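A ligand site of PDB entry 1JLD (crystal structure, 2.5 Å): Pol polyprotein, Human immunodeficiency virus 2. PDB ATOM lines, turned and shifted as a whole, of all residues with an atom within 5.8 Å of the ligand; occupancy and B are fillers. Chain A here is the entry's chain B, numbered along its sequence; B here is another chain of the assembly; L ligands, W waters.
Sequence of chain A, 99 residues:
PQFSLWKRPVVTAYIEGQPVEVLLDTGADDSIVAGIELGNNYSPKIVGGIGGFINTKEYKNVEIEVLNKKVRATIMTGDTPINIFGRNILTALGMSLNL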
ATOM      1  N   ARG A   8       4.922  18.577   1.355  1.00  0.00           N
ATOM      2  CA  ARG A   8       5.965  17.668   0.862  1.00  0.00           C
ATOM      3  C   ARG A   8       6.387  16.713   1.918  1.00  0.00           C
ATOM      4  O   ARG A   8       6.724  17.175   3.004  1.00  0.00           O
ATOM      5  CB  ARG A   8       7.222  18.429   0.495  1.00  0.00           C
ATOM      6  CG  ARG A   8       6.978  19.328  -0.697  1.00  0.00           C
ATOM      7  CD  ARG A   8       8.228  19.961  -1.123  1.00  0.00           C
ATOM      8  NE  ARG A   8       8.153  20.680  -2.378  1.00  0.00           N
ATOM      9  CZ  ARG A   8       9.242  21.353  -2.809  1.00  0.00           C
ATOM     10  NH1 ARG A   8      10.378  21.383  -2.069  1.00  0.00           N
ATOM     11  NH2 ARG A   8       9.202  22.003  -3.980  1.00  0.00           N
ATOM     12  N   LEU A  23      13.483  14.412   0.439  1.00  0.00           N
ATOM     13  CA  LEU A  23      12.180  14.201  -0.206  1.00  0.00           C
ATOM     14  C   LEU A  23      11.908  12.699  -0.353  1.00  0.00           C
ATOM     15  O   LEU A  23      12.755  12.036  -0.898  1.00  0.00           O
ATOM     16  CB  LEU A  23      12.310  14.753  -1.630  1.00  0.00           C
ATOM     17  CG  LEU A  23      11.209  15.648  -2.195  1.00  0.00           C
ATOM     18  CD1 LEU A  23      11.191  15.479  -3.705  1.00  0.00           C
ATOM     19  CD2 LEU A  23       9.836  15.330  -1.605  1.00  0.00           C
ATOM     20  N   ASP A  25      10.211  10.105  -2.443  1.00  0.00           N
ATOM     21  CA  ASP A  25       9.635  10.277  -3.754  1.00  0.00           C
ATOM     22  C   ASP A  25       9.363   8.997  -4.550  1.00  0.00           C
ATOM     23  O   ASP A  25      10.259   8.351  -5.068  1.00  0.00           O
ATOM     24  CB  ASP A  25      10.611  11.249  -4.488  1.00  0.00           C
ATOM     25  CG  ASP A  25      10.303  11.657  -5.891  1.00  0.00           C
ATOM     26  OD1 ASP A  25       9.219  11.549  -6.375  1.00  0.00           O
ATOM     27  OD2 ASP A  25      11.308  12.258  -6.469  1.00  0.00           O
ATOM     28  N   GLY A  27       8.207   8.756  -7.443  1.00  0.00           N
ATOM     29  CA  GLY A  27       8.436   8.987  -8.883  1.00  0.00           C
ATOM     30  C   GLY A  27       9.914   9.191  -9.167  1.00  0.00           C
ATOM     31  O   GLY A  27      10.286   9.659 -10.212  1.00  0.00           O
ATOM     32  N   ALA A  28      10.777   8.820  -8.216  1.00  0.00           N
ATOM     33  CA  ALA A  28      12.214   8.892  -8.369  1.00  0.00           C
ATOM     34  C   ALA A  28      12.804   7.498  -8.321  1.00  0.00           C
ATOM     35  O   ALA A  28      12.710   6.812  -7.286  1.00  0.00           O
ATOM     36  CB  ALA A  28      12.828   9.716  -7.247  1.00  0.00           C
ATOM     37  N   ASP A  29      13.411   7.071  -9.427  1.00  0.00           N
ATOM     38  CA  ASP A  29      14.041   5.779  -9.504  1.00  0.00           C
ATOM     39  C   ASP A  29      15.361   5.778  -8.775  1.00  0.00           C
ATOM     40  O   ASP A  29      15.741   4.786  -8.182  1.00  0.00           O
ATOM     41  CB  ASP A  29      14.333   5.392 -10.971  1.00  0.00           C
ATOM     42  CG  ASP A  29      13.163   5.062 -11.864  1.00  0.00           C
ATOM     43  OD1 ASP A  29      11.977   5.077 -11.288  1.00  0.00           O
ATOM     44  OD2 ASP A  29      13.326   4.795 -13.041  1.00  0.00           O
ATOM     45  N   ASP A  30      16.053   6.933  -8.806  1.00  0.00           N
ATOM     46  CA  ASP A  30      17.369   7.100  -8.157  1.00  0.00           C
ATOM     47  C   ASP A  30      17.275   7.983  -6.904  1.00  0.00           C
ATOM     48  O   ASP A  30      16.328   8.743  -6.747  1.00  0.00           O
ATOM     49  CB  ASP A  30      18.469   7.667  -9.127  1.00  0.00           C
ATOM     50  CG  ASP A  30      18.532   7.184 -10.592  1.00  0.00           C
ATOM     51  OD1 ASP A  30      19.250   6.121 -10.744  1.00  0.00           O
ATOM     52  OD2 ASP A  30      18.116   7.820 -11.558  1.00  0.00           O
ATOM     53  N   ILE A  32      19.184  11.046  -4.828  1.00  0.00           N
ATOM     54  CA  ILE A  32      20.183  12.043  -5.162  1.00  0.00           C
ATOM     55  C   ILE A  32      20.257  13.144  -4.121  1.00  0.00           C
ATOM     56  O   ILE A  32      19.223  13.603  -3.627  1.00  0.00           O
ATOM     57  CB  ILE A  32      19.858  12.532  -6.586  1.00  0.00           C
ATOM     58  CG1 ILE A  32      21.027  13.243  -7.260  1.00  0.00           C
ATOM     59  CG2 ILE A  32      18.583  13.388  -6.572  1.00  0.00           C
ATOM     60  CD1 ILE A  32      21.471  14.481  -6.498  1.00  0.00           C
ATOM     61  N   VAL A  47      21.870  12.149 -14.030  1.00  0.00           N
ATOM     62  CA  VAL A  47      20.524  11.957 -13.471  1.00  0.00           C
ATOM     63  C   VAL A  47      19.617  13.002 -14.124  1.00  0.00           C
ATOM     64  O   VAL A  47      20.057  14.119 -14.319  1.00  0.00           O
ATOM     65  CB  VAL A  47      20.460  11.835 -11.915  1.00  0.00           C
ATOM     66  CG1 VAL A  47      19.414  12.745 -11.270  1.00  0.00           C
ATOM     67  CG2 VAL A  47      20.048  10.425 -11.503  1.00  0.00           C
ATOM     68  N   GLY A  48      18.395  12.660 -14.548  1.00  0.00           N
ATOM     69  CA  GLY A  48      17.500  13.647 -15.187  1.00  0.00           C
ATOM     70  C   GLY A  48      16.069  13.694 -14.653  1.00  0.00           C
ATOM     71  O   GLY A  48      15.621  12.865 -13.885  1.00  0.00           O
ATOM     72  N   GLY A  49      15.328  14.728 -15.023  1.00  0.00           N
ATOM     73  CA  GLY A  49      13.950  14.847 -14.608  1.00  0.00           C
ATOM     74  C   GLY A  49      13.146  15.573 -15.660  1.00  0.00           C
ATOM     75  O   GLY A  49      13.032  15.135 -16.797  1.00  0.00           O
ATOM     76  N   ILE A  50      12.581  16.684 -15.248  1.00  0.00           N
ATOM     77  CA  ILE A  50      11.832  17.601 -16.079  1.00  0.00           C
ATOM     78  C   ILE A  50      12.815  18.745 -16.334  1.00  0.00           C
ATOM     79  O   ILE A  50      13.603  19.098 -15.454  1.00  0.00           O
ATOM     80  CB  ILE A  50      10.582  18.112 -15.300  1.00  0.00           C
ATOM     81  CG1 ILE A  50       9.250  17.529 -15.773  1.00  0.00           C
ATOM     82  CG2 ILE A  50      10.508  19.629 -15.164  1.00  0.00           C
ATOM     83  CD1 ILE A  50       8.510  16.825 -14.623  1.00  0.00           C
ATOM     84  N   GLY A  52      15.536  18.629 -17.869  1.00  0.00           N
ATOM     85  CA  GLY A  52      16.803  18.075 -18.380  1.00  0.00           C
ATOM     86  C   GLY A  52      17.568  17.086 -17.487  1.00  0.00           C
ATOM     87  O   GLY A  52      16.968  16.336 -16.759  1.00  0.00           O
ATOM     88  N   PHE A  53      18.921  17.115 -17.571  1.00  0.00           N
ATOM     89  CA  PHE A  53      19.762  16.208 -16.824  1.00  0.00           C
ATOM     90  C   PHE A  53      20.944  16.901 -16.194  1.00  0.00           C
ATOM     91  O   PHE A  53      21.328  17.939 -16.647  1.00  0.00           O
ATOM     92  CB  PHE A  53      20.335  15.066 -17.704  1.00  0.00           C
ATOM     93  CG  PHE A  53      19.308  14.282 -18.476  1.00  0.00           C
ATOM     94  CD1 PHE A  53      18.929  14.695 -19.752  1.00  0.00           C
ATOM     95  CD2 PHE A  53      18.759  13.120 -17.930  1.00  0.00           C
ATOM     96  CE1 PHE A  53      17.964  13.981 -20.469  1.00  0.00           C
ATOM     97  CE2 PHE A  53      17.800  12.398 -18.638  1.00  0.00           C
ATOM     98  CZ  PHE A  53      17.392  12.851 -19.891  1.00  0.00           C
ATOM     99  N   THR A  80      21.456  19.168  -7.021  1.00  0.00           N
ATOM    100  CA  THR A  80      20.005  19.090  -6.991  1.00  0.00           C
ATOM    101  C   THR A  80      19.529  20.199  -6.088  1.00  0.00           C
ATOM    102  O   THR A  80      20.181  20.511  -5.102  1.00  0.00           O
ATOM    103  CB  THR A  80      19.476  17.716  -6.512  1.00  0.00           C
ATOM    104  OG1 THR A  80      18.093  17.801  -6.263  1.00  0.00           O
ATOM    105  CG2 THR A  80      20.231  17.196  -5.285  1.00  0.00           C
ATOM    106  N   PRO A  81      18.400  20.803  -6.451  1.00  0.00           N
ATOM    107  CA  PRO A  81      17.823  21.876  -5.651  1.00  0.00           C
ATOM    108  C   PRO A  81      17.150  21.366  -4.360  1.00  0.00           C
ATOM    109  O   PRO A  81      16.810  22.165  -3.509  1.00  0.00           O
ATOM    110  CB  PRO A  81      16.728  22.479  -6.537  1.00  0.00           C
ATOM    111  CG  PRO A  81      16.537  21.597  -7.760  1.00  0.00           C
ATOM    112  CD  PRO A  81      17.616  20.518  -7.686  1.00  0.00           C
ATOM    113  N   ILE A  82      16.950  20.042  -4.246  1.00  0.00           N
ATOM    114  CA  ILE A  82      16.306  19.350  -3.149  1.00  0.00           C
ATOM    115  C   ILE A  82      16.908  17.924  -3.074  1.00  0.00           C
ATOM    116  O   ILE A  82      17.174  17.346  -4.123  1.00  0.00           O
ATOM    117  CB  ILE A  82      14.796  19.253  -3.500  1.00  0.00           C
ATOM    118  CG1 ILE A  82      14.140  20.645  -3.624  1.00  0.00           C
ATOM    119  CG2 ILE A  82      13.992  18.442  -2.500  1.00  0.00           C
ATOM    120  CD1 ILE A  82      13.868  21.267  -2.266  1.00  0.00           C
ATOM    121  N   ILE A  84      16.709  13.982  -2.649  1.00  0.00           N
ATOM    122  CA  ILE A  84      15.625  13.054  -2.929  1.00  0.00           C
ATOM    123  C   ILE A  84      15.958  11.626  -2.539  1.00  0.00           C
ATOM    124  O   ILE A  84      17.062  11.164  -2.806  1.00  0.00           O
ATOM    125  CB  ILE A  84      15.364  13.097  -4.438  1.00  0.00           C
ATOM    126  CG1 ILE A  84      14.662  14.367  -4.875  1.00  0.00           C
ATOM    127  CG2 ILE A  84      14.605  11.870  -4.926  1.00  0.00           C
ATOM    128  CD1 ILE A  84      14.967  14.768  -6.317  1.00  0.00           C
ATOM    129  N   ARG B   8       7.734   1.095 -10.705  1.00  0.00           N
ATOM    130  CA  ARG B   8       7.155   2.409 -10.632  1.00  0.00           C
ATOM    131  C   ARG B   8       5.670   2.327 -10.403  1.00  0.00           C
ATOM    132  O   ARG B   8       4.979   1.555 -11.099  1.00  0.00           O
ATOM    133  CB  ARG B   8       7.238   3.063 -11.955  1.00  0.00           C
ATOM    134  CG  ARG B   8       8.627   3.018 -12.502  1.00  0.00           C
ATOM    135  CD  ARG B   8       8.919   4.281 -13.295  1.00  0.00           C
ATOM    136  NE  ARG B   8      10.283   4.304 -13.753  1.00  0.00           N
ATOM    137  CZ  ARG B   8      10.545   4.333 -15.025  1.00  0.00           C
ATOM    138  NH1 ARG B   8       9.557   4.372 -15.928  1.00  0.00           N
ATOM    139  NH2 ARG B   8      11.817   4.331 -15.392  1.00  0.00           N
ATOM    140  N   LEU B  23       2.387   8.198 -13.574  1.00  0.00           N
ATOM    141  CA  LEU B  23       3.182   7.833 -12.445  1.00  0.00           C
ATOM    142  C   LEU B  23       2.621   8.591 -11.261  1.00  0.00           C
ATOM    143  O   LEU B  23       2.511   9.811 -11.350  1.00  0.00           O
ATOM    144  CB  LEU B  23       4.550   8.377 -12.753  1.00  0.00           C
ATOM    145  CG  LEU B  23       5.588   8.236 -11.678  1.00  0.00           C
ATOM    146  CD1 LEU B  23       5.658   6.799 -11.186  1.00  0.00           C
ATOM    147  CD2 LEU B  23       6.922   8.643 -12.289  1.00  0.00           C
ATOM    148  N   ASP B  25       3.203  10.340  -8.198  1.00  0.00           N
ATOM    149  CA  ASP B  25       4.413  10.984  -7.685  1.00  0.00           C
ATOM    150  C   ASP B  25       4.322  11.798  -6.400  1.00  0.00           C
ATOM    151  O   ASP B  25       4.046  12.982  -6.465  1.00  0.00           O
ATOM    152  CB  ASP B  25       4.973  11.916  -8.806  1.00  0.00           C
ATOM    153  CG  ASP B  25       6.453  12.252  -8.750  1.00  0.00           C
ATOM    154  OD1 ASP B  25       7.016  12.010  -7.600  1.00  0.00           O
ATOM    155  OD2 ASP B  25       7.044  12.823  -9.634  1.00  0.00           O
ATOM    156  N   GLY B  27       6.538  13.134  -5.058  1.00  0.00           N
ATOM    157  CA  GLY B  27       7.648  14.069  -5.160  1.00  0.00           C
ATOM    158  C   GLY B  27       7.417  15.204  -6.148  1.00  0.00           C
ATOM    159  O   GLY B  27       8.340  15.935  -6.512  1.00  0.00           O
ATOM    160  N   ALA B  28       6.142  15.350  -6.531  1.00  0.00           N
ATOM    161  CA  ALA B  28       5.712  16.385  -7.435  1.00  0.00           C
ATOM    162  C   ALA B  28       4.585  17.188  -6.780  1.00  0.00           C
ATOM    163  O   ALA B  28       3.534  16.662  -6.326  1.00  0.00           O
ATOM    164  CB  ALA B  28       5.262  15.716  -8.717  1.00  0.00           C
ATOM    165  N   ASP B  29       4.814  18.487  -6.703  1.00  0.00           N
ATOM    166  CA  ASP B  29       3.834  19.340  -6.122  1.00  0.00           C
ATOM    167  C   ASP B  29       2.697  19.517  -7.078  1.00  0.00           C
ATOM    168  O   ASP B  29       1.615  19.892  -6.638  1.00  0.00           O
ATOM    169  CB  ASP B  29       4.344  20.752  -5.970  1.00  0.00           C
ATOM    170  CG  ASP B  29       5.634  20.890  -5.256  1.00  0.00           C
ATOM    171  OD1 ASP B  29       6.071  20.092  -4.471  1.00  0.00           O
ATOM    172  OD2 ASP B  29       6.171  22.062  -5.508  1.00  0.00           O
ATOM    173  N   ASP B  30       3.035  19.373  -8.388  1.00  0.00           N
ATOM    174  CA  ASP B  30       2.092  19.552  -9.491  1.00  0.00           C
ATOM    175  C   ASP B  30       1.989  18.336 -10.469  1.00  0.00           C
ATOM    176  O   ASP B  30       2.860  17.454 -10.505  1.00  0.00           O
ATOM    177  CB  ASP B  30       2.359  20.911 -10.193  1.00  0.00           C
ATOM    178  CG  ASP B  30       2.364  22.103  -9.236  1.00  0.00           C
ATOM    179  OD1 ASP B  30       1.503  22.329  -8.356  1.00  0.00           O
ATOM    180  OD2 ASP B  30       3.412  22.889  -9.443  1.00  0.00           O
ATOM    181  N   ILE B  32       1.594  16.976 -14.387  1.00  0.00           N
ATOM    182  CA  ILE B  32       1.906  17.325 -15.755  1.00  0.00           C
ATOM    183  C   ILE B  32       1.771  16.116 -16.673  1.00  0.00           C
ATOM    184  O   ILE B  32       2.271  15.024 -16.419  1.00  0.00           O
ATOM    185  CB  ILE B  32       3.267  17.963 -15.910  1.00  0.00           C
ATOM    186  CG1 ILE B  32       3.565  18.028 -17.397  1.00  0.00           C
ATOM    187  CG2 ILE B  32       4.284  17.052 -15.262  1.00  0.00           C
ATOM    188  CD1 ILE B  32       4.682  18.984 -17.708  1.00  0.00           C
ATOM    189  N   VAL B  47       7.846  25.853 -15.243  1.00  0.00           N
ATOM    190  CA  VAL B  47       8.038  24.808 -14.286  1.00  0.00           C
ATOM    191  C   VAL B  47       9.443  24.280 -14.208  1.00  0.00           C
ATOM    192  O   VAL B  47      10.127  24.241 -15.237  1.00  0.00           O
ATOM    193  CB  VAL B  47       7.051  23.781 -14.794  1.00  0.00           C
ATOM    194  CG1 VAL B  47       7.587  22.387 -15.113  1.00  0.00           C
ATOM    195  CG2 VAL B  47       5.746  23.837 -14.018  1.00  0.00           C
ATOM    196  N   GLY B  48       9.805  23.826 -12.999  1.00  0.00           N
ATOM    197  CA  GLY B  48      11.120  23.262 -12.638  1.00  0.00           C
ATOM    198  C   GLY B  48      11.165  21.763 -12.217  1.00  0.00           C
ATOM    199  O   GLY B  48      10.244  21.185 -11.609  1.00  0.00           O
ATOM    200  N   GLY B  49      12.322  21.165 -12.600  1.00  0.00           N
ATOM    201  CA  GLY B  49      12.665  19.810 -12.331  1.00  0.00           C
ATOM    202  C   GLY B  49      14.121  19.797 -11.948  1.00  0.00           C
ATOM    203  O   GLY B  49      14.730  20.861 -11.825  1.00  0.00           O
ATOM    204  N   ILE B  50      14.677  18.595 -11.735  1.00  0.00           N
ATOM    205  CA  ILE B  50      16.098  18.415 -11.437  1.00  0.00           C
ATOM    206  C   ILE B  50      16.857  19.081 -12.570  1.00  0.00           C
ATOM    207  O   ILE B  50      17.744  19.920 -12.347  1.00  0.00           O
ATOM    208  CB  ILE B  50      16.475  16.916 -11.428  1.00  0.00           C
ATOM    209  CG1 ILE B  50      15.631  16.136 -10.447  1.00  0.00           C
ATOM    210  CG2 ILE B  50      17.938  16.677 -11.125  1.00  0.00           C
ATOM    211  CD1 ILE B  50      15.994  16.361  -8.977  1.00  0.00           C
ATOM    212  N   MET B  76      -1.259  20.317 -15.872  1.00  0.00           N
ATOM    213  CA  MET B  76      -0.471  21.184 -16.704  1.00  0.00           C
ATOM    214  C   MET B  76      -0.122  20.364 -17.930  1.00  0.00           C
ATOM    215  O   MET B  76      -0.114  19.148 -17.909  1.00  0.00           O
ATOM    216  CB  MET B  76       0.795  21.692 -16.032  1.00  0.00           C
ATOM    217  CG  MET B  76       0.521  22.342 -14.722  1.00  0.00           C
ATOM    218  SD  MET B  76       2.107  22.779 -13.987  1.00  0.00           S
ATOM    219  CE  MET B  76       2.150  24.518 -14.461  1.00  0.00           C
ATOM    220  N   THR B  80       6.975  16.133 -21.293  1.00  0.00           N
ATOM    221  CA  THR B  80       7.375  15.305 -20.172  1.00  0.00           C
ATOM    222  C   THR B  80       7.488  13.875 -20.647  1.00  0.00           C
ATOM    223  O   THR B  80       6.576  13.388 -21.311  1.00  0.00           O
ATOM    224  CB  THR B  80       6.449  15.473 -18.960  1.00  0.00           C
ATOM    225  OG1 THR B  80       6.998  14.766 -17.904  1.00  0.00           O
ATOM    226  CG2 THR B  80       5.036  14.965 -19.237  1.00  0.00           C
ATOM    227  N   PRO B  81       8.624  13.228 -20.391  1.00  0.00           N
ATOM    228  CA  PRO B  81       8.870  11.867 -20.817  1.00  0.00           C
ATOM    229  C   PRO B  81       7.876  10.874 -20.239  1.00  0.00           C
ATOM    230  O   PRO B  81       7.424   9.970 -20.946  1.00  0.00           O
ATOM    231  CB  PRO B  81      10.294  11.530 -20.408  1.00  0.00           C
ATOM    232  CG  PRO B  81      10.799  12.667 -19.535  1.00  0.00           C
ATOM    233  CD  PRO B  81       9.744  13.735 -19.538  1.00  0.00           C
ATOM    234  N   ILE B  82       7.547  11.028 -18.947  1.00  0.00           N
ATOM    235  CA  ILE B  82       6.559  10.200 -18.276  1.00  0.00           C
ATOM    236  C   ILE B  82       5.503  11.151 -17.779  1.00  0.00           C
ATOM    237  O   ILE B  82       5.862  12.285 -17.503  1.00  0.00           O
ATOM    238  CB  ILE B  82       7.200   9.355 -17.171  1.00  0.00           C
ATOM    239  CG1 ILE B  82       8.173   8.374 -17.809  1.00  0.00           C
ATOM    240  CG2 ILE B  82       6.193   8.593 -16.300  1.00  0.00           C
ATOM    241  CD1 ILE B  82       9.494   9.053 -18.103  1.00  0.00           C
ATOM    242  N   ILE B  84       2.877  12.685 -15.069  1.00  0.00           N
ATOM    243  CA  ILE B  84       2.921  12.578 -13.634  1.00  0.00           C
ATOM    244  C   ILE B  84       1.758  13.145 -12.861  1.00  0.00           C
ATOM    245  O   ILE B  84       1.313  14.272 -13.067  1.00  0.00           O
ATOM    246  CB  ILE B  84       4.293  13.027 -13.075  1.00  0.00           C
ATOM    247  CG1 ILE B  84       4.384  14.519 -13.093  1.00  0.00           C
ATOM    248  CG2 ILE B  84       5.480  12.486 -13.883  1.00  0.00           C
ATOM    249  CD1 ILE B  84       4.533  15.084 -11.683  1.00  0.00           C
HETATM  250  C1  LIG L   1      13.313   9.683 -12.778  1.00  0.00           C
HETATM  251  O1  LIG L   1      13.052   8.728 -12.003  1.00  0.00           O
HETATM  252  N1  LIG L   1      13.614  10.512 -15.064  1.00  0.00           N
HETATM  253  C2  LIG L   1      13.233   9.547 -14.197  1.00  0.00           C
HETATM  254  C3  LIG L   1      12.806   8.354 -14.769  1.00  0.00           C
HETATM  255  C4  LIG L   1      12.793   8.166 -16.140  1.00  0.00           C
HETATM  256  C5  LIG L   1      13.267   9.032 -18.358  1.00  0.00           C
HETATM  257  C6  LIG L   1      13.738  10.078 -19.148  1.00  0.00           C
HETATM  258  C7  LIG L   1      14.115  11.278 -18.568  1.00  0.00           C
HETATM  259  C8  LIG L   1      14.113  11.409 -17.196  1.00  0.00           C
HETATM  260  C9  LIG L   1      13.243   9.196 -16.963  1.00  0.00           C
HETATM  261  C10 LIG L   1      13.670  10.362 -16.405  1.00  0.00           C
HETATM  262  N2  LIG L   1      13.665  10.910 -12.339  1.00  0.00           N
HETATM  263  C11 LIG L   1      13.865  11.545 -11.037  1.00  0.00           C
HETATM  264  C12 LIG L   1      12.998  12.767 -11.037  1.00  0.00           C
HETATM  265  O2  LIG L   1      13.443  13.900 -11.189  1.00  0.00           O
HETATM  266  C13 LIG L   1      15.361  11.789 -10.607  1.00  0.00           C
HETATM  267  O3  LIG L   1      16.117  10.609 -10.742  1.00  0.00           O
HETATM  268  C14 LIG L   1      15.481  12.198  -9.149  1.00  0.00           C
HETATM  269  N3  LIG L   1      11.708  12.491 -10.931  1.00  0.00           N
HETATM  270  C15 LIG L   1      10.694  13.510 -11.048  1.00  0.00           C
HETATM  271  C16 LIG L   1      10.435  14.244  -9.725  1.00  0.00           C
HETATM  272  O4  LIG L   1       9.957  13.332  -8.767  1.00  0.00           O
HETATM  273  C17 LIG L   1       9.478  12.855 -11.695  1.00  0.00           C
HETATM  274  C18 LIG L   1       9.807  12.287 -13.041  1.00  0.00           C
HETATM  275  C19 LIG L   1      10.162  13.116 -14.110  1.00  0.00           C
HETATM  276  C20 LIG L   1       9.778  10.912 -13.266  1.00  0.00           C
HETATM  277  C21 LIG L   1      10.436  12.572 -15.366  1.00  0.00           C
HETATM  278  C22 LIG L   1      10.100  10.359 -14.510  1.00  0.00           C
HETATM  279  C23 LIG L   1      10.420  11.196 -15.580  1.00  0.00           C
HETATM  280  C24 LIG L   1       9.402  15.354  -9.832  1.00  0.00           C
HETATM  281  N4  LIG L   1       9.684  16.394  -8.845  1.00  0.00           N
HETATM  282  C25 LIG L   1      10.329  17.494  -9.150  1.00  0.00           C
HETATM  283  O5  LIG L   1      10.778  17.748 -10.258  1.00  0.00           O
HETATM  284  C26 LIG L   1      10.497  18.454  -7.980  1.00  0.00           C
HETATM  285  C27 LIG L   1      11.884  18.405  -7.212  1.00  0.00           C
HETATM  286  C28 LIG L   1      13.023  19.104  -7.950  1.00  0.00           C
HETATM  287  C29 LIG L   1      11.669  19.140  -5.906  1.00  0.00           C
HETATM  288  C30 LIG L   1      12.270  16.942  -6.995  1.00  0.00           C
HETATM  289  C31 LIG L   1      10.018  19.855  -8.414  1.00  0.00           C
HETATM  290  C32 LIG L   1       8.547  19.895  -8.774  1.00  0.00           C
HETATM  291  O6  LIG L   1       7.521  19.712  -7.909  1.00  0.00           O
HETATM  292  N5  LIG L   1       8.170  20.157 -10.040  1.00  0.00           N
HETATM  293  C33 LIG L   1       6.810  20.237 -10.457  1.00  0.00           C
HETATM  294  C34 LIG L   1       6.494  21.669 -10.876  1.00  0.00           C
HETATM  295  C35 LIG L   1       7.071  22.759  -9.933  1.00  0.00           C
HETATM  296  C36 LIG L   1       6.600  19.380 -11.698  1.00  0.00           C
HETATM  297  C37 LIG L   1       6.831  17.854 -11.530  1.00  0.00           C
HETATM  298  O   HOH W   1      12.414  16.508 -12.038  1.00  0.00           O
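OD1 of Asp 29 of chain B is in salt-bridge range of NE of Arg 8 of chain A (3.0 Å). OD1 of Asp 25 of chain A sits close to OD1 of Asp 25 of chain B. N of Ile 84 of chain A is in hydrogen-bond range of O of Ile 32 of chain A (2.7 Å). OD1 of Asp 25 of chain B sits at hydrogen-bond distance from N of Gly 27 of chain A (3.5 Å). The backbone NH (N) of Gly 27 of chain B sits close to the side-chain carboxylate (OD1) of Asp 25 of chain A, 3.4 Å away. The side-chain carboxylate of Asp 25 of chain B is in hydrogen-bond range of the backbone NH of Gly 27 of chain B (2.8 Å). The backbone NH (N) of Ile 84 of chain B is in hydrogen-bond range of the backbone carbonyl oxygen (O) of Ile 32 of chain B (2.8 Å). The backbone carbonyl oxygen (O) of Ile 82 of chain B is in hydrogen-bond range of the side-chain hydroxyl (OG1) of Thr 80 of chain B, 2.8 Å away.
Water W1 lies within hydrogen-bond range of an oxygen (O5) of the ligand (2.7 Å), the backbone NH (N) of Ile 50 of chain B (3.1 Å) and the backbone NH (N) of Ile 50 of chain A (3.2 Å).
Leu 23 of chain A touches the ligand (CD1 to C30, 3.8 Å). CA of Ala 28 of chain A touches O1 of the ligand (3.7 Å). Asp 30 of chain A touches the ligand (OD2 to O3, 3.5 Å). Val 47 of chain A touches the ligand. Gly 49 of chain A touches the ligand (CA to O2, 3.6 Å). Ile 50 of chain A touches the ligand. Phe 53 touches the ligand (CE2 to C7, 3.9 Å). CG1 of Ile 82 of chain A touches C29 of the ligand, at 3.7 Å. CD1 of Ile 84 of chain A touches C30 of the ligand, at 3.5 Å. Leu 23 of chain B touches the ligand (CD2 to C20, 3.8 Å). CA of Ala 28 of chain B touches O6 of the ligand (3.8 Å). Asp 30 of chain B touches the ligand (OD2 to C34, 3.6 Å). Val 47 of chain B touches the ligand. CA of Gly 49 of chain B touches O5 of the ligand (3.5 Å). Ile 50 of chain B touches the ligand. CG of Pro 81 of chain B touches C7 of the ligand, 3.7 Å away. Ile 82 of chain B touches the ligand. Ile 84 of chain B touches the ligand. Hydrophobic or aromatic side chains within 4 Å of the ligand: Leu 23 of chain A, Val 47 of chain A, Ile 50 of chain A, Phe 53, Ile 82 of chain A, Ile 84 of chain A, Leu 23 of chain B, Ala 28 of chain B, Val 47 of chain B, Ile 50 of chain B, Pro 81 of chain B, Ile 82 of chain B and Ile 84 of chain B. The nearest printed residue that does not touch the ligand is Arg 8 of chain B (4.03 Å).
O of Gly 27 of chain A is in hydrogen-bond range of N3 of the ligand. The backbone carbonyl oxygen (O) of Gly 48 of chain B lies within hydrogen-bond range of a nitrogen (N5) of the ligand (2.8 Å). The backbone NH (N) of Asp 29 of chain A is in hydrogen-bond range of an oxygen (O1) of the ligand, 3.1 Å away. OD2 of Asp 25 of chain A is in hydrogen-bond range of O4 of the ligand (2.9 Å). N4 of the ligand lies within hydrogen-bond range of O of Gly 27 of chain B, at 2.7 Å. A nitrogen (N2) of the ligand lies within hydrogen-bond range of the backbone carbonyl oxygen (O) of Gly 48 of chain A. The side-chain carboxylate (OD2) of Asp 25 of chain B lies within hydrogen-bond range of an oxygen (O4) of the ligand (3.1 Å). O6 of the ligand sits at hydrogen-bond distance from N of Asp 29 of chain B, 3.2 Å away.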
